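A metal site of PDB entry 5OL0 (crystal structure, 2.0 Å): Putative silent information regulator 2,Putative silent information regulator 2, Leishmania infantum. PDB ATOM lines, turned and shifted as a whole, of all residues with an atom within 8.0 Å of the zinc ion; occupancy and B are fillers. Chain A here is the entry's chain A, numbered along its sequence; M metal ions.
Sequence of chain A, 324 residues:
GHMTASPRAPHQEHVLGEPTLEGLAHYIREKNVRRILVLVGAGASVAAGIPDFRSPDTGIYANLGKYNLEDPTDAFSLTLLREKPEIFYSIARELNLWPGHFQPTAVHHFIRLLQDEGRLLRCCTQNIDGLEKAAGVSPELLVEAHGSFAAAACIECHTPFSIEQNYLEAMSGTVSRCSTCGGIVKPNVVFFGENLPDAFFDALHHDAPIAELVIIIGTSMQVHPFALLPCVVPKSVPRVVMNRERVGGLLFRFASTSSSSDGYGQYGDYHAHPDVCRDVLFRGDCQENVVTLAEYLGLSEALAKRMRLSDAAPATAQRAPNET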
ATOM      1  N   ALA A 153     -23.440  29.498 -16.578  1.00  0.00           N
ATOM      2  CA  ALA A 153     -23.190  28.755 -17.828  1.00  0.00           C
ATOM      3  C   ALA A 153     -22.071  27.741 -17.669  1.00  0.00           C
ATOM      4  O   ALA A 153     -21.195  27.898 -16.803  1.00  0.00           O
ATOM      5  CB  ALA A 153     -22.846  29.746 -18.985  1.00  0.00           C
ATOM      6  N   CYS A 154     -22.114  26.703 -18.496  1.00  0.00           N
ATOM      7  CA  CYS A 154     -20.983  25.753 -18.604  1.00  0.00           C
ATOM      8  C   CYS A 154     -19.712  26.386 -19.136  1.00  0.00           C
ATOM      9  O   CYS A 154     -19.736  27.096 -20.128  1.00  0.00           O
ATOM     10  CB  CYS A 154     -21.344  24.639 -19.585  1.00  0.00           C
ATOM     11  SG  CYS A 154     -20.056  23.370 -19.723  1.00  0.00           S
ATOM     12  N   ILE A 155     -18.595  26.162 -18.468  1.00  0.00           N
ATOM     13  CA  ILE A 155     -17.324  26.716 -18.962  1.00  0.00           C
ATOM     14  C   ILE A 155     -16.792  25.976 -20.211  1.00  0.00           C
ATOM     15  O   ILE A 155     -16.018  26.550 -20.939  1.00  0.00           O
ATOM     16  CB  ILE A 155     -16.207  26.721 -17.877  1.00  0.00           C
ATOM     17  CG1 ILE A 155     -15.679  25.291 -17.646  1.00  0.00           C
ATOM     18  CG2 ILE A 155     -16.696  27.452 -16.595  1.00  0.00           C
ATOM     19  CD1 ILE A 155     -14.630  25.164 -16.575  1.00  0.00           C
ATOM     20  N   GLU A 156     -17.150  24.698 -20.425  1.00  0.00           N
ATOM     21  CA  GLU A 156     -16.670  23.949 -21.607  1.00  0.00           C
ATOM     22  C   GLU A 156     -17.499  24.314 -22.856  1.00  0.00           C
ATOM     23  O   GLU A 156     -16.936  24.800 -23.829  1.00  0.00           O
ATOM     24  CB  GLU A 156     -16.643  22.403 -21.369  1.00  0.00           C
ATOM     25  CG  GLU A 156     -15.788  21.826 -20.212  1.00  0.00           C
ATOM     26  CD  GLU A 156     -14.403  22.447 -19.968  1.00  0.00           C
ATOM     27  OE1 GLU A 156     -13.804  23.166 -20.827  1.00  0.00           O
ATOM     28  OE2 GLU A 156     -13.852  22.205 -18.867  1.00  0.00           O
ATOM     29  N   CYS A 157     -18.816  24.090 -22.836  1.00  0.00           N
ATOM     30  CA  CYS A 157     -19.678  24.367 -24.004  1.00  0.00           C
ATOM     31  C   CYS A 157     -20.474  25.659 -23.983  1.00  0.00           C
ATOM     32  O   CYS A 157     -21.199  25.931 -24.930  1.00  0.00           O
ATOM     33  CB  CYS A 157     -20.644  23.181 -24.233  1.00  0.00           C
ATOM     34  SG  CYS A 157     -22.047  23.019 -23.080  1.00  0.00           S
ATOM     35  N   HIS A 158     -20.376  26.462 -22.913  1.00  0.00           N
ATOM     36  CA  HIS A 158     -21.088  27.756 -22.814  1.00  0.00           C
ATOM     37  C   HIS A 158     -22.645  27.689 -22.803  1.00  0.00           C
ATOM     38  O   HIS A 158     -23.326  28.720 -22.881  1.00  0.00           O
ATOM     39  CB  HIS A 158     -20.515  28.752 -23.830  1.00  0.00           C
ATOM     40  CG  HIS A 158     -19.027  28.961 -23.685  1.00  0.00           C
ATOM     41  ND1 HIS A 158     -18.472  29.600 -22.599  1.00  0.00           N
ATOM     42  CD2 HIS A 158     -17.996  28.557 -24.452  1.00  0.00           C
ATOM     43  CE1 HIS A 158     -17.153  29.592 -22.708  1.00  0.00           C
ATOM     44  NE2 HIS A 158     -16.835  28.963 -23.828  1.00  0.00           N
ATOM     45  N   THR A 159     -23.209  26.497 -22.610  1.00  0.00           N
ATOM     46  CA  THR A 159     -24.676  26.352 -22.511  1.00  0.00           C
ATOM     47  C   THR A 159     -25.177  26.954 -21.173  1.00  0.00           C
ATOM     48  O   THR A 159     -24.734  26.481 -20.093  1.00  0.00           O
ATOM     49  CB  THR A 159     -25.139  24.877 -22.515  1.00  0.00           C
ATOM     50  OG1 THR A 159     -24.674  24.228 -23.701  1.00  0.00           O
ATOM     51  CG2 THR A 159     -26.678  24.762 -22.419  1.00  0.00           C
ATOM     52  N   PRO A 160     -26.143  27.903 -21.236  1.00  0.00           N
ATOM     53  CA  PRO A 160     -26.739  28.451 -20.014  1.00  0.00           C
ATOM     54  C   PRO A 160     -27.264  27.385 -19.072  1.00  0.00           C
ATOM     55  O   PRO A 160     -27.647  26.281 -19.499  1.00  0.00           O
ATOM     56  CB  PRO A 160     -27.893  29.308 -20.535  1.00  0.00           C
ATOM     57  CG  PRO A 160     -27.422  29.746 -21.884  1.00  0.00           C
ATOM     58  CD  PRO A 160     -26.781  28.502 -22.423  1.00  0.00           C
ATOM     59  N   ARG A 177     -23.050  21.141 -12.652  1.00  0.00           N
ATOM     60  CA  ARG A 177     -22.548  20.442 -13.836  1.00  0.00           C
ATOM     61  C   ARG A 177     -23.506  20.568 -14.988  1.00  0.00           C
ATOM     62  O   ARG A 177     -24.719  20.468 -14.800  1.00  0.00           O
ATOM     63  CB  ARG A 177     -22.359  18.950 -13.524  1.00  0.00           C
ATOM     64  CG  ARG A 177     -21.257  18.652 -12.539  1.00  0.00           C
ATOM     65  CD  ARG A 177     -19.942  18.611 -13.303  1.00  0.00           C
ATOM     66  NE  ARG A 177     -18.757  18.361 -12.488  1.00  0.00           N
ATOM     67  CZ  ARG A 177     -17.507  18.234 -12.974  1.00  0.00           C
ATOM     68  NH1 ARG A 177     -17.257  18.340 -14.284  1.00  0.00           N
ATOM     69  NH2 ARG A 177     -16.495  18.033 -12.136  1.00  0.00           N
ATOM     70  N   CYS A 178     -22.960  20.799 -16.178  1.00  0.00           N
ATOM     71  CA  CYS A 178     -23.679  20.946 -17.419  1.00  0.00           C
ATOM     72  C   CYS A 178     -24.486  19.681 -17.733  1.00  0.00           C
ATOM     73  O   CYS A 178     -23.968  18.589 -17.576  1.00  0.00           O
ATOM     74  CB  CYS A 178     -22.658  21.125 -18.525  1.00  0.00           C
ATOM     75  SG  CYS A 178     -23.287  21.605 -20.136  1.00  0.00           S
ATOM     76  N   SER A 179     -25.720  19.827 -18.209  1.00  0.00           N
ATOM     77  CA  SER A 179     -26.556  18.660 -18.589  1.00  0.00           C
ATOM     78  C   SER A 179     -26.390  18.281 -20.069  1.00  0.00           C
ATOM     79  O   SER A 179     -27.167  17.492 -20.602  1.00  0.00           O
ATOM     80  CB  SER A 179     -28.026  18.979 -18.325  1.00  0.00           C
ATOM     81  OG  SER A 179     -28.197  19.514 -17.023  1.00  0.00           O
ATOM     82  N   THR A 180     -25.405  18.879 -20.741  1.00  0.00           N
ATOM     83  CA  THR A 180     -25.068  18.574 -22.116  1.00  0.00           C
ATOM     84  C   THR A 180     -23.736  17.818 -22.166  1.00  0.00           C
ATOM     85  O   THR A 180     -23.660  16.756 -22.783  1.00  0.00           O
ATOM     86  CB  THR A 180     -25.014  19.847 -22.984  1.00  0.00           C
ATOM     87  OG1 THR A 180     -26.345  20.390 -23.105  1.00  0.00           O
ATOM     88  CG2 THR A 180     -24.432  19.565 -24.382  1.00  0.00           C
ATOM     89  N   CYS A 181     -22.697  18.333 -21.493  1.00  0.00           N
ATOM     90  CA  CYS A 181     -21.332  17.796 -21.604  1.00  0.00           C
ATOM     91  C   CYS A 181     -20.698  17.359 -20.291  1.00  0.00           C
ATOM     92  O   CYS A 181     -19.534  16.933 -20.269  1.00  0.00           O
ATOM     93  CB  CYS A 181     -20.447  18.862 -22.286  1.00  0.00           C
ATOM     94  SG  CYS A 181     -19.795  20.182 -21.196  1.00  0.00           S
ATOM     95  N   GLY A 182     -21.430  17.484 -19.172  1.00  0.00           N
ATOM     96  CA  GLY A 182     -20.831  17.247 -17.878  1.00  0.00           C
ATOM     97  C   GLY A 182     -19.740  18.248 -17.485  1.00  0.00           C
ATOM     98  O   GLY A 182     -19.063  18.076 -16.465  1.00  0.00           O
ATOM     99  N   GLY A 183     -19.568  19.324 -18.256  1.00  0.00           N
ATOM    100  CA  GLY A 183     -18.673  20.373 -17.838  1.00  0.00           C
ATOM    101  C   GLY A 183     -19.068  21.055 -16.519  1.00  0.00           C
ATOM    102  O   GLY A 183     -20.210  20.963 -16.046  1.00  0.00           O
ATOM    103  N   ILE A 184     -18.092  21.699 -15.929  1.00  0.00           N
ATOM    104  CA  ILE A 184     -18.284  22.501 -14.739  1.00  0.00           C
ATOM    105  C   ILE A 184     -19.016  23.807 -15.051  1.00  0.00           C
ATOM    106  O   ILE A 184     -18.617  24.532 -15.988  1.00  0.00           O
ATOM    107  CB  ILE A 184     -16.945  22.869 -14.094  1.00  0.00           C
ATOM    108  CG1 ILE A 184     -16.321  21.639 -13.423  1.00  0.00           C
ATOM    109  CG2 ILE A 184     -17.142  23.969 -13.027  1.00  0.00           C
ATOM    110  CD1 ILE A 184     -14.801  21.728 -13.342  1.00  0.00           C
ATOM    111  N   VAL A 185     -20.053  24.091 -14.277  1.00  0.00           N
ATOM    112  CA  VAL A 185     -20.851  25.330 -14.430  1.00  0.00           C
ATOM    113  C   VAL A 185     -20.352  26.317 -13.378  1.00  0.00           C
ATOM    114  O   VAL A 185     -19.910  25.945 -12.242  1.00  0.00           O
ATOM    115  CB  VAL A 185     -22.355  25.035 -14.316  1.00  0.00           C
ATOM    116  CG1 VAL A 185     -23.201  26.302 -14.051  1.00  0.00           C
ATOM    117  CG2 VAL A 185     -22.838  24.363 -15.610  1.00  0.00           C
HETATM  118 ZN    ZN M   1     -21.249  22.016 -21.195  1.00  0.00          ZN
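Of the 17 residues printed, 4 come within 4 Å of the zinc ion.
The side-chain sulfur (SG) of Cys 181 lies close to the backbone NH (N) of Gly 183 (3.1 Å). The backbone NH of Glu 156 sits close to the side-chain sulfur of Cys 154 (3.3 Å). SG of Cys 178 sits close to N of Thr 180, 3.5 Å away. The backbone NH (N) of Cys 154 sits at hydrogen-bond distance from the backbone carbonyl oxygen (O) of Thr 159, 3.1 Å away. The side-chain sulfur of Cys 157 lies close to the side-chain hydroxyl of Thr 159 (3.0 Å). The backbone NH (N) of Cys 178 lies within hydrogen-bond range of the backbone carbonyl oxygen (O) of Gly 183 (2.8 Å).
The zinc ion is bound by the side-chain sulfur of Cys 157 (2.3 Å), the side-chain sulfur of Cys 154 (2.3 Å), the side-chain sulfur of Cys 178 (2.3 Å) and the side-chain sulfur of Cys 181 (2.3 Å). The zinc ion has four donor atoms within binding distance.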
